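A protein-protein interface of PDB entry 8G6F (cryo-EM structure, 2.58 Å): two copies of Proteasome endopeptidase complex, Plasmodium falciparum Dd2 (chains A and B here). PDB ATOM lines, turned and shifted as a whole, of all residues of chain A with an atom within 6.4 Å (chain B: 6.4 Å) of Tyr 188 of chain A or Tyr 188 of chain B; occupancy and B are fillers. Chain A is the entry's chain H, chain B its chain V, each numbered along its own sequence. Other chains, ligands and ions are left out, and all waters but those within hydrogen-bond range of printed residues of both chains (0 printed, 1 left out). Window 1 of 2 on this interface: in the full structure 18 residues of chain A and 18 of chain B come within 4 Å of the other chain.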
ATOM      1  N   SER A 184     -12.558  -6.456  27.618  1.00  0.00           N
ATOM      2  CA  SER A 184     -12.006  -5.132  27.871  1.00  0.00           C
ATOM      3  C   SER A 184     -11.136  -4.650  26.718  1.00  0.00           C
ATOM      4  O   SER A 184     -11.063  -3.444  26.465  1.00  0.00           O
ATOM      5  CB  SER A 184     -11.202  -5.147  29.168  1.00  0.00           C
ATOM      6  OG  SER A 184     -10.396  -6.307  29.248  1.00  0.00           O
ATOM      7  N   GLY A 185     -10.473  -5.565  26.011  1.00  0.00           N
ATOM      8  CA  GLY A 185      -9.556  -5.168  24.960  1.00  0.00           C
ATOM      9  C   GLY A 185     -10.212  -4.795  23.652  1.00  0.00           C
ATOM     10  O   GLY A 185      -9.569  -4.153  22.815  1.00  0.00           O
ATOM     11  N   SER A 186     -11.473  -5.179  23.452  1.00  0.00           N
ATOM     12  CA  SER A 186     -12.145  -4.898  22.188  1.00  0.00           C
ATOM     13  C   SER A 186     -12.338  -3.404  21.967  1.00  0.00           C
ATOM     14  O   SER A 186     -12.402  -2.947  20.817  1.00  0.00           O
ATOM     15  CB  SER A 186     -13.492  -5.609  22.154  1.00  0.00           C
ATOM     16  OG  SER A 186     -14.283  -5.260  23.273  1.00  0.00           O
ATOM     17  N   ILE A 187     -12.435  -2.633  23.048  1.00  0.00           N
ATOM     18  CA  ILE A 187     -12.660  -1.200  22.913  1.00  0.00           C
ATOM     19  C   ILE A 187     -11.531  -0.565  22.117  1.00  0.00           C
ATOM     20  O   ILE A 187     -11.760   0.308  21.275  1.00  0.00           O
ATOM     21  CB  ILE A 187     -12.809  -0.549  24.302  1.00  0.00           C
ATOM     22  CG1 ILE A 187     -13.870  -1.275  25.136  1.00  0.00           C
ATOM     23  CG2 ILE A 187     -13.175   0.915  24.169  1.00  0.00           C
ATOM     24  CD1 ILE A 187     -15.280  -1.192  24.579  1.00  0.00           C
ATOM     25  N   TYR A 188     -10.296  -1.005  22.359  1.00  0.00           N
ATOM     26  CA  TYR A 188      -9.143  -0.393  21.716  1.00  0.00           C
ATOM     27  C   TYR A 188      -9.090  -0.673  20.223  1.00  0.00           C
ATOM     28  O   TYR A 188      -8.484   0.107  19.484  1.00  0.00           O
ATOM     29  CB  TYR A 188      -7.861  -0.881  22.386  1.00  0.00           C
ATOM     30  CG  TYR A 188      -7.846  -0.662  23.880  1.00  0.00           C
ATOM     31  CD1 TYR A 188      -7.754   0.611  24.414  1.00  0.00           C
ATOM     32  CD2 TYR A 188      -7.935  -1.728  24.754  1.00  0.00           C
ATOM     33  CE1 TYR A 188      -7.746   0.810  25.770  1.00  0.00           C
ATOM     34  CE2 TYR A 188      -7.926  -1.537  26.108  1.00  0.00           C
ATOM     35  CZ  TYR A 188      -7.831  -0.267  26.613  1.00  0.00           C
ATOM     36  OH  TYR A 188      -7.826  -0.077  27.972  1.00  0.00           O
ATOM     37  N   ILE A 189      -9.709  -1.757  19.762  1.00  0.00           N
ATOM     38  CA  ILE A 189      -9.686  -2.141  18.358  1.00  0.00           C
ATOM     39  C   ILE A 189     -11.029  -1.901  17.685  1.00  0.00           C
ATOM     40  O   ILE A 189     -11.221  -2.309  16.538  1.00  0.00           O
ATOM     41  CB  ILE A 189      -9.258  -3.607  18.187  1.00  0.00           C
ATOM     42  CG1 ILE A 189     -10.085  -4.514  19.101  1.00  0.00           C
ATOM     43  CG2 ILE A 189      -7.784  -3.759  18.474  1.00  0.00           C
ATOM     44  CD1 ILE A 189     -10.540  -5.783  18.447  1.00  0.00           C
ATOM     45  N   GLN A 190     -11.970  -1.258  18.375  1.00  0.00           N
ATOM     46  CA  GLN A 190     -13.290  -1.035  17.793  1.00  0.00           C
ATOM     47  C   GLN A 190     -13.210  -0.348  16.432  1.00  0.00           C
ATOM     48  O   GLN A 190     -13.782  -0.830  15.450  1.00  0.00           O
ATOM     49  CB  GLN A 190     -14.144  -0.211  18.755  1.00  0.00           C
ATOM     50  CG  GLN A 190     -15.613  -0.163  18.396  1.00  0.00           C
ATOM     51  CD  GLN A 190     -16.179  -1.533  18.102  1.00  0.00           C
ATOM     52  OE1 GLN A 190     -15.879  -2.498  18.799  1.00  0.00           O
ATOM     53  NE2 GLN A 190     -16.997  -1.628  17.064  1.00  0.00           N
ATOM     54  N   SER A 191     -12.510   0.783  16.350  1.00  0.00           N
ATOM     55  CA  SER A 191     -12.451   1.527  15.095  1.00  0.00           C
ATOM     56  C   SER A 191     -11.540   0.863  14.075  1.00  0.00           C
ATOM     57  O   SER A 191     -11.773   0.981  12.869  1.00  0.00           O
ATOM     58  CB  SER A 191     -11.978   2.955  15.349  1.00  0.00           C
ATOM     59  OG  SER A 191     -12.830   3.615  16.263  1.00  0.00           O
ATOM     60  N   TYR A 192     -10.500   0.176  14.539  1.00  0.00           N
ATOM     61  CA  TYR A 192      -9.604  -0.533  13.637  1.00  0.00           C
ATOM     62  C   TYR A 192     -10.356  -1.603  12.854  1.00  0.00           C
ATOM     63  O   TYR A 192     -10.248  -1.689  11.624  1.00  0.00           O
ATOM     64  CB  TYR A 192      -8.468  -1.143  14.457  1.00  0.00           C
ATOM     65  CG  TYR A 192      -7.538  -2.042  13.695  1.00  0.00           C
ATOM     66  CD1 TYR A 192      -6.418  -1.535  13.065  1.00  0.00           C
ATOM     67  CD2 TYR A 192      -7.769  -3.405  13.621  1.00  0.00           C
ATOM     68  CE1 TYR A 192      -5.565  -2.354  12.375  1.00  0.00           C
ATOM     69  CE2 TYR A 192      -6.920  -4.229  12.932  1.00  0.00           C
ATOM     70  CZ  TYR A 192      -5.818  -3.699  12.313  1.00  0.00           C
ATOM     71  OH  TYR A 192      -4.962  -4.515  11.621  1.00  0.00           O
ATOM     72  N   TYR A 216      -3.476  -6.068  18.523  1.00  0.00           N
ATOM     73  CA  TYR A 216      -3.620  -4.681  18.956  1.00  0.00           C
ATOM     74  C   TYR A 216      -4.313  -4.596  20.310  1.00  0.00           C
ATOM     75  O   TYR A 216      -3.910  -3.806  21.178  1.00  0.00           O
ATOM     76  CB  TYR A 216      -4.394  -3.890  17.907  1.00  0.00           C
ATOM     77  CG  TYR A 216      -3.515  -3.301  16.835  1.00  0.00           C
ATOM     78  CD1 TYR A 216      -2.677  -2.234  17.110  1.00  0.00           C
ATOM     79  CD2 TYR A 216      -3.517  -3.815  15.552  1.00  0.00           C
ATOM     80  CE1 TYR A 216      -1.870  -1.696  16.138  1.00  0.00           C
ATOM     81  CE2 TYR A 216      -2.713  -3.286  14.573  1.00  0.00           C
ATOM     82  CZ  TYR A 216      -1.892  -2.225  14.871  1.00  0.00           C
ATOM     83  OH  TYR A 216      -1.086  -1.690  13.896  1.00  0.00           O
ATOM     84  N   ALA A 217      -5.352  -5.406  20.514  1.00  0.00           N
ATOM     85  CA  ALA A 217      -6.035  -5.400  21.799  1.00  0.00           C
ATOM     86  C   ALA A 217      -5.089  -5.794  22.922  1.00  0.00           C
ATOM     87  O   ALA A 217      -5.100  -5.183  23.995  1.00  0.00           O
ATOM     88  CB  ALA A 217      -7.237  -6.335  21.757  1.00  0.00           C
ATOM     89  N   ASN A 220      -2.640  -2.948  23.767  1.00  0.00           N
ATOM     90  CA  ASN A 220      -3.175  -1.782  24.459  1.00  0.00           C
ATOM     91  C   ASN A 220      -3.831  -2.099  25.796  1.00  0.00           C
ATOM     92  O   ASN A 220      -4.015  -1.183  26.603  1.00  0.00           O
ATOM     93  CB  ASN A 220      -4.191  -1.070  23.568  1.00  0.00           C
ATOM     94  CG  ASN A 220      -3.538  -0.298  22.453  1.00  0.00           C
ATOM     95  OD1 ASN A 220      -3.780  -0.558  21.279  1.00  0.00           O
ATOM     96  ND2 ASN A 220      -2.703   0.664  22.814  1.00  0.00           N
ATOM     97  N   ASP A 221      -4.183  -3.353  26.060  1.00  0.00           N
ATOM     98  CA  ASP A 221      -4.960  -3.725  27.236  1.00  0.00           C
ATOM     99  C   ASP A 221      -4.110  -4.565  28.177  1.00  0.00           C
ATOM    100  O   ASP A 221      -3.492  -5.546  27.753  1.00  0.00           O
ATOM    101  CB  ASP A 221      -6.215  -4.498  26.822  1.00  0.00           C
ATOM    102  CG  ASP A 221      -7.200  -4.673  27.959  1.00  0.00           C
ATOM    103  OD1 ASP A 221      -7.403  -3.724  28.739  1.00  0.00           O
ATOM    104  OD2 ASP A 221      -7.776  -5.770  28.069  1.00  0.00           O
ATOM    105  N   ASN A 222      -4.085  -4.181  29.454  1.00  0.00           N
ATOM    106  CA  ASN A 222      -3.323  -4.925  30.448  1.00  0.00           C
ATOM    107  C   ASN A 222      -3.976  -6.250  30.802  1.00  0.00           C
ATOM    108  O   ASN A 222      -3.282  -7.172  31.241  1.00  0.00           O
ATOM    109  CB  ASN A 222      -3.160  -4.096  31.721  1.00  0.00           C
ATOM    110  CG  ASN A 222      -2.056  -3.077  31.616  1.00  0.00           C
ATOM    111  OD1 ASN A 222      -1.169  -3.189  30.775  1.00  0.00           O
ATOM    112  ND2 ASN A 222      -2.099  -2.076  32.477  1.00  0.00           N
ATOM    113  N   SER B 184     -12.921  10.366  26.332  1.00  0.00           N
ATOM    114  CA  SER B 184     -13.562   9.058  26.343  1.00  0.00           C
ATOM    115  C   SER B 184     -13.532   8.400  24.970  1.00  0.00           C
ATOM    116  O   SER B 184     -13.488   7.171  24.878  1.00  0.00           O
ATOM    117  CB  SER B 184     -15.001   9.192  26.832  1.00  0.00           C
ATOM    118  OG  SER B 184     -15.616  10.338  26.278  1.00  0.00           O
ATOM    119  N   GLY B 185     -13.555   9.193  23.898  1.00  0.00           N
ATOM    120  CA  GLY B 185     -13.618   8.631  22.562  1.00  0.00           C
ATOM    121  C   GLY B 185     -12.296   8.144  22.018  1.00  0.00           C
ATOM    122  O   GLY B 185     -12.285   7.387  21.044  1.00  0.00           O
ATOM    123  N   SER B 186     -11.181   8.560  22.620  1.00  0.00           N
ATOM    124  CA  SER B 186      -9.871   8.162  22.117  1.00  0.00           C
ATOM    125  C   SER B 186      -9.646   6.663  22.244  1.00  0.00           C
ATOM    126  O   SER B 186      -8.890   6.076  21.455  1.00  0.00           O
ATOM    127  CB  SER B 186      -8.781   8.920  22.867  1.00  0.00           C
ATOM    128  OG  SER B 186      -8.896   8.727  24.265  1.00  0.00           O
ATOM    129  N   ILE B 187     -10.284   6.030  23.226  1.00  0.00           N
ATOM    130  CA  ILE B 187     -10.085   4.601  23.435  1.00  0.00           C
ATOM    131  C   ILE B 187     -10.484   3.829  22.188  1.00  0.00           C
ATOM    132  O   ILE B 187      -9.811   2.873  21.792  1.00  0.00           O
ATOM    133  CB  ILE B 187     -10.873   4.127  24.670  1.00  0.00           C
ATOM    134  CG1 ILE B 187     -10.525   4.973  25.899  1.00  0.00           C
ATOM    135  CG2 ILE B 187     -10.588   2.667  24.954  1.00  0.00           C
ATOM    136  CD1 ILE B 187      -9.104   4.799  26.400  1.00  0.00           C
ATOM    137  N   TYR B 188     -11.575   4.241  21.543  1.00  0.00           N
ATOM    138  CA  TYR B 188     -12.088   3.508  20.395  1.00  0.00           C
ATOM    139  C   TYR B 188     -11.174   3.605  19.183  1.00  0.00           C
ATOM    140  O   TYR B 188     -11.208   2.715  18.329  1.00  0.00           O
ATOM    141  CB  TYR B 188     -13.482   4.017  20.040  1.00  0.00           C
ATOM    142  CG  TYR B 188     -14.447   3.972  21.201  1.00  0.00           C
ATOM    143  CD1 TYR B 188     -14.906   2.766  21.702  1.00  0.00           C
ATOM    144  CD2 TYR B 188     -14.891   5.135  21.799  1.00  0.00           C
ATOM    145  CE1 TYR B 188     -15.776   2.724  22.759  1.00  0.00           C
ATOM    146  CE2 TYR B 188     -15.760   5.102  22.853  1.00  0.00           C
ATOM    147  CZ  TYR B 188     -16.203   3.896  23.331  1.00  0.00           C
ATOM    148  OH  TYR B 188     -17.074   3.864  24.391  1.00  0.00           O
ATOM    149  N   ILE B 189     -10.356   4.650  19.091  1.00  0.00           N
ATOM    150  CA  ILE B 189      -9.460   4.854  17.959  1.00  0.00           C
ATOM    151  C   ILE B 189      -8.015   4.574  18.307  1.00  0.00           C
ATOM    152  O   ILE B 189      -7.135   4.811  17.470  1.00  0.00           O
ATOM    153  CB  ILE B 189      -9.594   6.278  17.391  1.00  0.00           C
ATOM    154  CG1 ILE B 189      -9.452   7.311  18.509  1.00  0.00           C
ATOM    155  CG2 ILE B 189     -10.912   6.436  16.675  1.00  0.00           C
ATOM    156  CD1 ILE B 189      -8.708   8.547  18.106  1.00  0.00           C
ATOM    157  N   GLN B 190      -7.733   4.100  19.521  1.00  0.00           N
ATOM    158  CA  GLN B 190      -6.356   3.817  19.912  1.00  0.00           C
ATOM    159  C   GLN B 190      -5.619   2.989  18.863  1.00  0.00           C
ATOM    160  O   GLN B 190      -4.598   3.420  18.320  1.00  0.00           O
ATOM    161  CB  GLN B 190      -6.346   3.101  21.264  1.00  0.00           C
ATOM    162  CG  GLN B 190      -5.007   3.119  21.973  1.00  0.00           C
ATOM    163  CD  GLN B 190      -4.360   4.486  21.959  1.00  0.00           C
ATOM    164  OE1 GLN B 190      -4.999   5.486  22.273  1.00  0.00           O
ATOM    165  NE2 GLN B 190      -3.088   4.537  21.590  1.00  0.00           N
ATOM    166  N   SER B 191      -6.114   1.784  18.571  1.00  0.00           N
ATOM    167  CA  SER B 191      -5.406   0.900  17.648  1.00  0.00           C
ATOM    168  C   SER B 191      -5.443   1.420  16.220  1.00  0.00           C
ATOM    169  O   SER B 191      -4.510   1.180  15.449  1.00  0.00           O
ATOM    170  CB  SER B 191      -6.000  -0.504  17.706  1.00  0.00           C
ATOM    171  OG  SER B 191      -5.982  -1.004  19.027  1.00  0.00           O
ATOM    172  N   TYR B 192      -6.513   2.116  15.846  1.00  0.00           N
ATOM    173  CA  TYR B 192      -6.613   2.677  14.505  1.00  0.00           C
ATOM    174  C   TYR B 192      -5.493   3.678  14.250  1.00  0.00           C
ATOM    175  O   TYR B 192      -4.802   3.616  13.225  1.00  0.00           O
ATOM    176  CB  TYR B 192      -7.984   3.332  14.347  1.00  0.00           C
ATOM    177  CG  TYR B 192      -8.182   4.094  13.067  1.00  0.00           C
ATOM    178  CD1 TYR B 192      -8.672   3.466  11.938  1.00  0.00           C
ATOM    179  CD2 TYR B 192      -7.894   5.446  12.991  1.00  0.00           C
ATOM    180  CE1 TYR B 192      -8.859   4.158  10.771  1.00  0.00           C
ATOM    181  CE2 TYR B 192      -8.079   6.143  11.827  1.00  0.00           C
ATOM    182  CZ  TYR B 192      -8.562   5.494  10.720  1.00  0.00           C
ATOM    183  OH  TYR B 192      -8.752   6.183   9.550  1.00  0.00           O
ATOM    184  N   TYR B 216     -14.211   8.492  13.684  1.00  0.00           N
ATOM    185  CA  TYR B 216     -14.433   7.177  14.277  1.00  0.00           C
ATOM    186  C   TYR B 216     -14.756   7.286  15.760  1.00  0.00           C
ATOM    187  O   TYR B 216     -15.649   6.588  16.264  1.00  0.00           O
ATOM    188  CB  TYR B 216     -13.207   6.298  14.057  1.00  0.00           C
ATOM    189  CG  TYR B 216     -13.237   5.546  12.751  1.00  0.00           C
ATOM    190  CD1 TYR B 216     -14.109   4.488  12.560  1.00  0.00           C
ATOM    191  CD2 TYR B 216     -12.401   5.899  11.708  1.00  0.00           C
ATOM    192  CE1 TYR B 216     -14.144   3.803  11.372  1.00  0.00           C
ATOM    193  CE2 TYR B 216     -12.429   5.222  10.516  1.00  0.00           C
ATOM    194  CZ  TYR B 216     -13.302   4.173  10.351  1.00  0.00           C
ATOM    195  OH  TYR B 216     -13.335   3.491   9.160  1.00  0.00           O
ATOM    196  N   ALA B 217     -14.047   8.159  16.475  1.00  0.00           N
ATOM    197  CA  ALA B 217     -14.331   8.339  17.892  1.00  0.00           C
ATOM    198  C   ALA B 217     -15.757   8.824  18.104  1.00  0.00           C
ATOM    199  O   ALA B 217     -16.452   8.349  19.009  1.00  0.00           O
ATOM    200  CB  ALA B 217     -13.335   9.314  18.506  1.00  0.00           C
ATOM    201  N   ASN B 220     -18.305   5.992  17.547  1.00  0.00           N
ATOM    202  CA  ASN B 220     -18.380   4.944  18.557  1.00  0.00           C
ATOM    203  C   ASN B 220     -18.709   5.449  19.956  1.00  0.00           C
ATOM    204  O   ASN B 220     -19.135   4.649  20.794  1.00  0.00           O
ATOM    205  CB  ASN B 220     -17.061   4.175  18.609  1.00  0.00           C
ATOM    206  CG  ASN B 220     -16.881   3.258  17.430  1.00  0.00           C
ATOM    207  OD1 ASN B 220     -15.979   3.442  16.620  1.00  0.00           O
ATOM    208  ND2 ASN B 220     -17.745   2.262  17.323  1.00  0.00           N
ATOM    209  N   ASP B 221     -18.536   6.736  20.232  1.00  0.00           N
ATOM    210  CA  ASP B 221     -18.663   7.279  21.578  1.00  0.00           C
ATOM    211  C   ASP B 221     -19.875   8.195  21.658  1.00  0.00           C
ATOM    212  O   ASP B 221     -20.036   9.092  20.825  1.00  0.00           O
ATOM    213  CB  ASP B 221     -17.395   8.044  21.966  1.00  0.00           C
ATOM    214  CG  ASP B 221     -17.346   8.397  23.439  1.00  0.00           C
ATOM    215  OD1 ASP B 221     -17.706   7.550  24.278  1.00  0.00           O
ATOM    216  OD2 ASP B 221     -16.935   9.526  23.758  1.00  0.00           O
ATOM    217  N   ASN B 222     -20.723   7.968  22.662  1.00  0.00           N
ATOM    218  CA  ASN B 222     -21.906   8.798  22.850  1.00  0.00           C
ATOM    219  C   ASN B 222     -21.563  10.182  23.372  1.00  0.00           C
ATOM    220  O   ASN B 222     -22.342  11.118  23.170  1.00  0.00           O
ATOM    221  CB  ASN B 222     -22.876   8.126  23.821  1.00  0.00           C
ATOM    222  CG  ASN B 222     -23.700   7.047  23.170  1.00  0.00           C
ATOM    223  OD1 ASN B 222     -23.819   6.990  21.950  1.00  0.00           O
ATOM    224  ND2 ASN B 222     -24.280   6.182  23.984  1.00  0.00           N
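The backbone carbonyl oxygen of Ile 187 of chain A lies close to the backbone carbonyl oxygen of Ile 187 of chain B (3.3 Å).
The side-chain hydroxyl (OG) of Ser 191 of chain B lies within hydrogen-bond range of the side-chain amide oxygen (OD1) of Asn 220 of chain A, at 3.2 Å.
O of Tyr 188 of chain A is in hydrogen-bond range of OG of Ser 191 of chain B (2.8 Å).
The backbone carbonyl oxygen (O) of Tyr 188 of chain B is in hydrogen-bond range of the side-chain hydroxyl (OG) of Ser 191 of chain A, at 2.8 Å.
OD1 of Asn 220 of chain B sits at hydrogen-bond distance from OG of Ser 191 of chain A (3.2 Å).
The backbone carbonyl oxygen of Tyr 216 of chain B sits close to the side-chain amide oxygen of Asn 220 of chain B (3.2 Å).
O of Tyr 216 of chain A sits close to OD1 of Asn 220 of chain A (3.3 Å).
Among the printed residues, pairs that only touch across the chains: Ile 187 of chain A with Tyr 188 of chain B (3.3 Å), Tyr 188 of chain A with Ile 187 of chain B (3.3 Å), Tyr 188 of chain A with Tyr 188 of chain B (3.9 Å), Ile 189 of chain A with Ser 191 of chain B (3.3 Å), Gln 190 of chain A with Asn 220 of chain B (3.4 Å), Ser 191 of chain A with Ile 189 of chain B (3.4 Å), Ser 191 of chain A with Tyr 216 of chain B (3.5 Å), Tyr 216 of chain A with Ser 191 of chain B (3.5 Å) and Asn 220 of chain A with Gln 190 of chain B (3.5 Å).
Tyr 188 of chain A touches three residues of chain B.
Tyr 188 of chain B touches just these residues of chain A: Ile 187, Tyr 188 and Ser 191.
Printed residues of chain B within 4 Å of Ile 187 of chain A: Ile 187 (3.2 Å) and Tyr 188 (3.3 Å).
Printed residues of chain A within 4 Å of Tyr 216 of chain B: Ser 191.
Tyr 192 of chain B touches none of the printed residues of chain A.
Tyr 192 of chain A touches none of the printed residues of chain B.
The nearest residue of chain A that does not touch Tyr 188 of chain B is Gln 190 of chain A (4.05 Å).
Hydrophobic or aromatic side chains of chain B within 4 Å of the printed part of chain A: Ile 187, Tyr 188, Ile 189 and Tyr 216.
Hydrophobic or aromatic side chains of chain A within 4 Å of the printed part of chain B: Ile 187, Tyr 188, Ile 189 and Tyr 216.
Tyr 188 of chain B touches its own counterpart, Tyr 188 of chain A.
Gln 190 of chain A touches Asn 220 of chain B, and with the chains exchanged Asn 220 of chain A touches Gln 190 of chain B.
Ser 191 of chain A touches Tyr 216 of chain B, and with the chains exchanged Tyr 216 of chain A touches Ser 191 of chain B.
Ser 191 of chain A touches Asn 220 of chain B, and with the chains exchanged Asn 220 of chain A touches Ser 191 of chain B.
Positions printed for both chains: 184, 185, 186, 187, 188, 189, 190, 191, 192, 216, 217, 220, 221 and 222.
Of the 14 pairs that touch across the chains among the printed residues, 14 have their exchanged pair printed and touching as well.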
